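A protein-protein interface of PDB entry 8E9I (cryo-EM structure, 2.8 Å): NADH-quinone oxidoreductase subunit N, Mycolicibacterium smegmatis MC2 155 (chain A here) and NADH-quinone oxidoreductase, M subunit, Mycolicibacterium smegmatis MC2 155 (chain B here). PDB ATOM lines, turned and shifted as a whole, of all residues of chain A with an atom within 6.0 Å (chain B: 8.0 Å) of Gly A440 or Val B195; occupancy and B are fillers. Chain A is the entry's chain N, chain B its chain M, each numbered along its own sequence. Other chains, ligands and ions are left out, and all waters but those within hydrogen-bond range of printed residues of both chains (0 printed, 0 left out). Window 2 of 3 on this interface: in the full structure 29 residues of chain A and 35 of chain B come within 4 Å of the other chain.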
ATOM      1  N   VAL A 435     -27.346  14.238   3.860  1.00  0.00           N
ATOM      2  CA  VAL A 435     -27.184  14.336   5.310  1.00  0.00           C
ATOM      3  C   VAL A 435     -26.669  13.018   5.881  1.00  0.00           C
ATOM      4  O   VAL A 435     -25.777  13.005   6.737  1.00  0.00           O
ATOM      5  CB  VAL A 435     -28.490  14.775   5.993  1.00  0.00           C
ATOM      6  CG1 VAL A 435     -28.811  16.210   5.622  1.00  0.00           C
ATOM      7  CG2 VAL A 435     -29.627  13.857   5.634  1.00  0.00           C
ATOM      8  N   PHE A 436     -27.217  11.891   5.427  1.00  0.00           N
ATOM      9  CA  PHE A 436     -26.762  10.600   5.927  1.00  0.00           C
ATOM     10  C   PHE A 436     -25.302  10.354   5.578  1.00  0.00           C
ATOM     11  O   PHE A 436     -24.554   9.791   6.381  1.00  0.00           O
ATOM     12  CB  PHE A 436     -27.639   9.486   5.358  1.00  0.00           C
ATOM     13  CG  PHE A 436     -29.048   9.477   5.883  1.00  0.00           C
ATOM     14  CD1 PHE A 436     -29.400  10.184   7.021  1.00  0.00           C
ATOM     15  CD2 PHE A 436     -30.026   8.759   5.225  1.00  0.00           C
ATOM     16  CE1 PHE A 436     -30.694  10.163   7.490  1.00  0.00           C
ATOM     17  CE2 PHE A 436     -31.321   8.737   5.694  1.00  0.00           C
ATOM     18  CZ  PHE A 436     -31.652   9.444   6.828  1.00  0.00           C
ATOM     19  N   LYS A 437     -24.883  10.747   4.376  1.00  0.00           N
ATOM     20  CA  LYS A 437     -23.490  10.581   3.984  1.00  0.00           C
ATOM     21  C   LYS A 437     -22.582  11.401   4.882  1.00  0.00           C
ATOM     22  O   LYS A 437     -21.530  10.927   5.320  1.00  0.00           O
ATOM     23  CB  LYS A 437     -23.307  10.993   2.526  1.00  0.00           C
ATOM     24  CG  LYS A 437     -21.907  10.768   1.984  1.00  0.00           C
ATOM     25  CD  LYS A 437     -21.683  11.527   0.694  1.00  0.00           C
ATOM     26  CE  LYS A 437     -21.375  12.985   0.970  1.00  0.00           C
ATOM     27  NZ  LYS A 437     -19.912  13.213   1.099  1.00  0.00           N
ATOM     28  N   ALA A 438     -22.971  12.641   5.166  1.00  0.00           N
ATOM     29  CA  ALA A 438     -22.175  13.452   6.077  1.00  0.00           C
ATOM     30  C   ALA A 438     -22.095  12.803   7.448  1.00  0.00           C
ATOM     31  O   ALA A 438     -21.024  12.759   8.061  1.00  0.00           O
ATOM     32  CB  ALA A 438     -22.761  14.853   6.187  1.00  0.00           C
ATOM     33  N   ALA A 439     -23.219  12.293   7.949  1.00  0.00           N
ATOM     34  CA  ALA A 439     -23.221  11.681   9.272  1.00  0.00           C
ATOM     35  C   ALA A 439     -22.321  10.454   9.313  1.00  0.00           C
ATOM     36  O   ALA A 439     -21.539  10.279  10.254  1.00  0.00           O
ATOM     37  CB  ALA A 439     -24.645  11.312   9.676  1.00  0.00           C
ATOM     38  N   GLY A 440     -22.416   9.593   8.302  1.00  0.00           N
ATOM     39  CA  GLY A 440     -21.568   8.413   8.277  1.00  0.00           C
ATOM     40  C   GLY A 440     -20.101   8.766   8.143  1.00  0.00           C
ATOM     41  O   GLY A 440     -19.254   8.246   8.871  1.00  0.00           O
ATOM     42  N   GLU A 441     -19.782   9.670   7.218  1.00  0.00           N
ATOM     43  CA  GLU A 441     -18.400  10.097   7.049  1.00  0.00           C
ATOM     44  C   GLU A 441     -17.875  10.772   8.305  1.00  0.00           C
ATOM     45  O   GLU A 441     -16.661  10.794   8.537  1.00  0.00           O
ATOM     46  CB  GLU A 441     -18.288  11.036   5.849  1.00  0.00           C
ATOM     47  N   GLY A 442     -18.764  11.329   9.121  1.00  0.00           N
ATOM     48  CA  GLY A 442     -18.383  11.956  10.364  1.00  0.00           C
ATOM     49  C   GLY A 442     -18.291  11.026  11.547  1.00  0.00           C
ATOM     50  O   GLY A 442     -18.061  11.484  12.668  1.00  0.00           O
ATOM     51  N   GLY A 443     -18.456   9.724  11.336  1.00  0.00           N
ATOM     52  CA  GLY A 443     -18.430   8.761  12.411  1.00  0.00           C
ATOM     53  C   GLY A 443     -19.785   8.398  12.977  1.00  0.00           C
ATOM     54  O   GLY A 443     -19.863   7.490  13.812  1.00  0.00           O
ATOM     55  N   ALA A 444     -20.850   9.077  12.561  1.00  0.00           N
ATOM     56  CA  ALA A 444     -22.202   8.800  13.048  1.00  0.00           C
ATOM     57  C   ALA A 444     -22.978   7.869  12.130  1.00  0.00           C
ATOM     58  O   ALA A 444     -24.101   8.183  11.726  1.00  0.00           O
ATOM     59  CB  ALA A 444     -22.948  10.116  13.235  1.00  0.00           C
ATOM     60  N   ILE A 445     -22.414   6.721  11.776  1.00  0.00           N
ATOM     61  CA  ILE A 445     -23.105   5.744  10.938  1.00  0.00           C
ATOM     62  C   ILE A 445     -24.340   5.230  11.670  1.00  0.00           C
ATOM     63  O   ILE A 445     -25.394   5.050  11.040  1.00  0.00           O
ATOM     64  CB  ILE A 445     -22.173   4.593  10.535  1.00  0.00           C
ATOM     65  CG1 ILE A 445     -20.976   5.134   9.753  1.00  0.00           C
ATOM     66  CG2 ILE A 445     -22.923   3.580   9.677  1.00  0.00           C
ATOM     67  CD1 ILE A 445     -19.853   4.139   9.583  1.00  0.00           C
ATOM     68  N   VAL A 448     -27.143   7.020  10.717  1.00  0.00           N
ATOM     69  CA  VAL A 448     -27.605   6.709   9.370  1.00  0.00           C
ATOM     70  C   VAL A 448     -28.509   5.489   9.395  1.00  0.00           C
ATOM     71  O   VAL A 448     -29.531   5.445   8.706  1.00  0.00           O
ATOM     72  CB  VAL A 448     -26.420   6.504   8.416  1.00  0.00           C
ATOM     73  CG1 VAL A 448     -26.938   6.042   7.067  1.00  0.00           C
ATOM     74  CG2 VAL A 448     -25.628   7.785   8.281  1.00  0.00           C
ATOM     75  N   ALA B 188     -28.490   2.502   3.517  1.00  0.00           N
ATOM     76  CA  ALA B 188     -27.543   2.437   4.621  1.00  0.00           C
ATOM     77  C   ALA B 188     -26.240   1.805   4.160  1.00  0.00           C
ATOM     78  O   ALA B 188     -25.150   2.337   4.401  1.00  0.00           O
ATOM     79  CB  ALA B 188     -28.142   1.641   5.777  1.00  0.00           C
ATOM     80  N   ALA B 189     -26.344   0.670   3.470  1.00  0.00           N
ATOM     81  CA  ALA B 189     -25.155  -0.011   2.972  1.00  0.00           C
ATOM     82  C   ALA B 189     -24.399   0.832   1.954  1.00  0.00           C
ATOM     83  O   ALA B 189     -23.168   0.811   1.929  1.00  0.00           O
ATOM     84  CB  ALA B 189     -25.546  -1.347   2.355  1.00  0.00           C
ATOM     85  N   VAL B 190     -25.112   1.553   1.095  1.00  0.00           N
ATOM     86  CA  VAL B 190     -24.470   2.366   0.070  1.00  0.00           C
ATOM     87  C   VAL B 190     -23.660   3.474   0.719  1.00  0.00           C
ATOM     88  O   VAL B 190     -22.526   3.763   0.319  1.00  0.00           O
ATOM     89  CB  VAL B 190     -25.529   2.932  -0.893  1.00  0.00           C
ATOM     90  CG1 VAL B 190     -24.952   4.065  -1.713  1.00  0.00           C
ATOM     91  CG2 VAL B 190     -26.055   1.839  -1.797  1.00  0.00           C
ATOM     92  N   ILE B 191     -24.235   4.113   1.734  1.00  0.00           N
ATOM     93  CA  ILE B 191     -23.527   5.184   2.420  1.00  0.00           C
ATOM     94  C   ILE B 191     -22.341   4.620   3.191  1.00  0.00           C
ATOM     95  O   ILE B 191     -21.272   5.238   3.252  1.00  0.00           O
ATOM     96  CB  ILE B 191     -24.500   5.954   3.325  1.00  0.00           C
ATOM     97  CG1 ILE B 191     -25.498   6.702   2.445  1.00  0.00           C
ATOM     98  CG2 ILE B 191     -23.744   6.913   4.230  1.00  0.00           C
ATOM     99  CD1 ILE B 191     -26.594   7.387   3.192  1.00  0.00           C
ATOM    100  N   GLY B 192     -22.500   3.433   3.775  1.00  0.00           N
ATOM    101  CA  GLY B 192     -21.364   2.786   4.410  1.00  0.00           C
ATOM    102  C   GLY B 192     -20.250   2.492   3.424  1.00  0.00           C
ATOM    103  O   GLY B 192     -19.069   2.675   3.724  1.00  0.00           O
ATOM    104  N   LEU B 193     -20.613   2.026   2.233  1.00  0.00           N
ATOM    105  CA  LEU B 193     -19.618   1.773   1.199  1.00  0.00           C
ATOM    106  C   LEU B 193     -18.914   3.057   0.796  1.00  0.00           C
ATOM    107  O   LEU B 193     -17.697   3.062   0.582  1.00  0.00           O
ATOM    108  CB  LEU B 193     -20.277   1.131  -0.017  1.00  0.00           C
ATOM    109  CG  LEU B 193     -19.352   0.920  -1.213  1.00  0.00           C
ATOM    110  CD1 LEU B 193     -18.258  -0.080  -0.883  1.00  0.00           C
ATOM    111  CD2 LEU B 193     -20.156   0.480  -2.416  1.00  0.00           C
ATOM    112  N   TYR B 194     -19.665   4.147   0.664  1.00  0.00           N
ATOM    113  CA  TYR B 194     -19.044   5.419   0.323  1.00  0.00           C
ATOM    114  C   TYR B 194     -18.053   5.837   1.397  1.00  0.00           C
ATOM    115  O   TYR B 194     -16.947   6.298   1.096  1.00  0.00           O
ATOM    116  CB  TYR B 194     -20.102   6.500   0.135  1.00  0.00           C
ATOM    117  CG  TYR B 194     -19.498   7.811  -0.288  1.00  0.00           C
ATOM    118  CD1 TYR B 194     -19.015   8.709   0.650  1.00  0.00           C
ATOM    119  CD2 TYR B 194     -19.388   8.141  -1.626  1.00  0.00           C
ATOM    120  CE1 TYR B 194     -18.452   9.901   0.267  1.00  0.00           C
ATOM    121  CE2 TYR B 194     -18.824   9.330  -2.018  1.00  0.00           C
ATOM    122  CZ  TYR B 194     -18.359  10.205  -1.070  1.00  0.00           C
ATOM    123  OH  TYR B 194     -17.794  11.393  -1.466  1.00  0.00           O
ATOM    124  N   VAL B 195     -18.437   5.682   2.664  1.00  0.00           N
ATOM    125  CA  VAL B 195     -17.543   6.045   3.757  1.00  0.00           C
ATOM    126  C   VAL B 195     -16.287   5.187   3.722  1.00  0.00           C
ATOM    127  O   VAL B 195     -15.169   5.684   3.903  1.00  0.00           O
ATOM    128  CB  VAL B 195     -18.271   5.920   5.105  1.00  0.00           C
ATOM    129  CG1 VAL B 195     -17.289   6.037   6.252  1.00  0.00           C
ATOM    130  CG2 VAL B 195     -19.349   6.981   5.219  1.00  0.00           C
ATOM    131  N   VAL B 196     -16.450   3.885   3.494  1.00  0.00           N
ATOM    132  CA  VAL B 196     -15.299   2.992   3.472  1.00  0.00           C
ATOM    133  C   VAL B 196     -14.360   3.364   2.333  1.00  0.00           C
ATOM    134  O   VAL B 196     -13.141   3.445   2.518  1.00  0.00           O
ATOM    135  CB  VAL B 196     -15.769   1.531   3.375  1.00  0.00           C
ATOM    136  CG1 VAL B 196     -14.595   0.600   3.159  1.00  0.00           C
ATOM    137  CG2 VAL B 196     -16.503   1.138   4.635  1.00  0.00           C
ATOM    138  N   THR B 197     -14.906   3.602   1.142  1.00  0.00           N
ATOM    139  CA  THR B 197     -14.067   4.010   0.020  1.00  0.00           C
ATOM    140  C   THR B 197     -13.351   5.314   0.328  1.00  0.00           C
ATOM    141  O   THR B 197     -12.175   5.480  -0.006  1.00  0.00           O
ATOM    142  CB  THR B 197     -14.910   4.166  -1.240  1.00  0.00           C
ATOM    143  OG1 THR B 197     -15.990   5.072  -0.980  1.00  0.00           O
ATOM    144  CG2 THR B 197     -15.475   2.831  -1.670  1.00  0.00           C
ATOM    145  N   ALA B 198     -14.051   6.258   0.959  1.00  0.00           N
ATOM    146  CA  ALA B 198     -13.420   7.518   1.329  1.00  0.00           C
ATOM    147  C   ALA B 198     -12.338   7.304   2.379  1.00  0.00           C
ATOM    148  O   ALA B 198     -11.374   8.071   2.453  1.00  0.00           O
ATOM    149  CB  ALA B 198     -14.476   8.497   1.836  1.00  0.00           C
ATOM    150  N   GLY B 199     -12.481   6.266   3.202  1.00  0.00           N
ATOM    151  CA  GLY B 199     -11.499   5.991   4.233  1.00  0.00           C
ATOM    152  C   GLY B 199     -10.294   5.202   3.764  1.00  0.00           C
ATOM    153  O   GLY B 199      -9.360   5.011   4.550  1.00  0.00           O
ATOM    154  N   SER B 200     -10.287   4.750   2.514  1.00  0.00           N
ATOM    155  CA  SER B 200      -9.226   3.904   1.990  1.00  0.00           C
ATOM    156  C   SER B 200      -8.418   4.664   0.949  1.00  0.00           C
ATOM    157  O   SER B 200      -8.955   5.494   0.210  1.00  0.00           O
ATOM    158  CB  SER B 200      -9.799   2.629   1.374  1.00  0.00           C
ATOM    159  OG  SER B 200      -8.764   1.771   0.932  1.00  0.00           O
ATOM    160  N   ALA B 205     -11.160   9.571  -3.900  1.00  0.00           N
ATOM    161  CA  ALA B 205     -12.179  10.120  -3.020  1.00  0.00           C
ATOM    162  C   ALA B 205     -13.300   9.099  -2.918  1.00  0.00           C
ATOM    163  O   ALA B 205     -13.342   8.124  -3.669  1.00  0.00           O
ATOM    164  CB  ALA B 205     -12.695  11.464  -3.537  1.00  0.00           C
ATOM    165  N   GLY B 206     -14.206   9.331  -1.975  1.00  0.00           N
ATOM    166  CA  GLY B 206     -15.350   8.455  -1.833  1.00  0.00           C
ATOM    167  C   GLY B 206     -15.984   8.211  -3.183  1.00  0.00           C
ATOM    168  O   GLY B 206     -16.450   9.149  -3.834  1.00  0.00           O
ATOM    169  N   THR B 207     -16.006   6.956  -3.616  1.00  0.00           N
ATOM    170  CA  THR B 207     -16.315   6.630  -4.996  1.00  0.00           C
ATOM    171  C   THR B 207     -17.513   5.699  -5.053  1.00  0.00           C
ATOM    172  O   THR B 207     -17.747   4.903  -4.140  1.00  0.00           O
ATOM    173  CB  THR B 207     -15.117   5.973  -5.689  1.00  0.00           C
ATOM    174  OG1 THR B 207     -14.007   6.875  -5.682  1.00  0.00           O
ATOM    175  CG2 THR B 207     -15.454   5.620  -7.118  1.00  0.00           C
ATOM    176  N   PHE B 208     -18.282   5.824  -6.133  1.00  0.00           N
ATOM    177  CA  PHE B 208     -19.339   4.880  -6.449  1.00  0.00           C
ATOM    178  C   PHE B 208     -19.117   4.172  -7.777  1.00  0.00           C
ATOM    179  O   PHE B 208     -19.888   3.265  -8.107  1.00  0.00           O
ATOM    180  CB  PHE B 208     -20.708   5.578  -6.485  1.00  0.00           C
ATOM    181  CG  PHE B 208     -21.275   5.893  -5.130  1.00  0.00           C
ATOM    182  CD1 PHE B 208     -21.403   4.911  -4.169  1.00  0.00           C
ATOM    183  CD2 PHE B 208     -21.715   7.168  -4.832  1.00  0.00           C
ATOM    184  CE1 PHE B 208     -21.933   5.202  -2.935  1.00  0.00           C
ATOM    185  CE2 PHE B 208     -22.250   7.462  -3.598  1.00  0.00           C
ATOM    186  CZ  PHE B 208     -22.362   6.479  -2.652  1.00  0.00           C
ATOM    187  N   PHE B 222      -7.922  -2.330  -1.978  1.00  0.00           N
ATOM    188  CA  PHE B 222      -9.061  -1.883  -1.180  1.00  0.00           C
ATOM    189  C   PHE B 222      -9.335  -2.883  -0.056  1.00  0.00           C
ATOM    190  O   PHE B 222     -10.392  -3.505   0.035  1.00  0.00           O
ATOM    191  CB  PHE B 222     -10.273  -1.698  -2.083  1.00  0.00           C
ATOM    192  CG  PHE B 222     -11.455  -1.042  -1.418  1.00  0.00           C
ATOM    193  CD1 PHE B 222     -11.309  -0.294  -0.265  1.00  0.00           C
ATOM    194  CD2 PHE B 222     -12.715  -1.156  -1.974  1.00  0.00           C
ATOM    195  CE1 PHE B 222     -12.397   0.309   0.323  1.00  0.00           C
ATOM    196  CE2 PHE B 222     -13.802  -0.556  -1.389  1.00  0.00           C
ATOM    197  CZ  PHE B 222     -13.644   0.178  -0.239  1.00  0.00           C
ATOM    198  N   ILE B 228     -16.892  -4.874   8.574  1.00  0.00           N
ATOM    199  CA  ILE B 228     -17.575  -3.836   7.810  1.00  0.00           C
ATOM    200  C   ILE B 228     -18.069  -4.402   6.487  1.00  0.00           C
ATOM    201  O   ILE B 228     -19.189  -4.118   6.046  1.00  0.00           O
ATOM    202  CB  ILE B 228     -16.650  -2.625   7.601  1.00  0.00           C
ATOM    203  CG1 ILE B 228     -16.575  -1.793   8.886  1.00  0.00           C
ATOM    204  CG2 ILE B 228     -17.120  -1.786   6.416  1.00  0.00           C
ATOM    205  CD1 ILE B 228     -15.526  -0.694   8.856  1.00  0.00           C
ATOM    206  N   LEU B 232     -21.961  -4.451   5.181  1.00  0.00           N
ATOM    207  CA  LEU B 232     -22.373  -3.836   3.924  1.00  0.00           C
ATOM    208  C   LEU B 232     -22.956  -4.878   2.977  1.00  0.00           C
ATOM    209  O   LEU B 232     -23.951  -4.624   2.283  1.00  0.00           O
ATOM    210  CB  LEU B 232     -21.191  -3.113   3.279  1.00  0.00           C
ATOM    211  CG  LEU B 232     -20.559  -1.966   4.071  1.00  0.00           C
ATOM    212  CD1 LEU B 232     -19.577  -1.173   3.201  1.00  0.00           C
ATOM    213  CD2 LEU B 232     -21.628  -1.062   4.659  1.00  0.00           C
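O of Tyr B194 is in hydrogen-bond range of OG1 of Thr B197, at 2.6 Å.
Among the printed residues, pairs that only touch across the chains: Phe A436 with Ile B191, Glu A441 with Val B195, Gly A440 with Val B195, Lys A437 with Tyr B194 and Lys A437 with Ile B191.
Printed residues of chain B within 4 Å of Phe A436: Ile B191 (3.2 Å).
Printed residues of chain B within 4 Å of Lys A437: Ile B191 and Tyr B194.
No residue of chain B comes within 4 Å of Ala A439.
Gly A440 touches just one residue of chain B: Val B195.
Of chain B, only Val B195 (3.4 Å) comes within 4 Å of Glu A441.
Gly A442 touches none of the printed residues of chain B.
Of the printed residues of chain A, Tyr B194 touches Lys A437 (3.6 Å).
Val B195 touches just these residues of chain A: Gly A440 (3.5 Å) and Glu A441 (3.4 Å).
Phe B208 touches none of the printed residues of chain A.
Hydrophobic or aromatic side chains of chain B that line the printed part of chain A: Ile B191, Tyr B194 and Val B195.
Of the 12 printed residues of chain A, 4 touch a printed residue of chain B.
Hydrophobic or aromatic side chains of chain A within 4 Å of the printed part of chain B: Phe A436.
Among the printed residues, 5 pairs touch across the chains.
Among the printed residues, no Asp or Glu carboxylate lies within 4 Å of a Lys or Arg side-chain nitrogen of the other chain.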
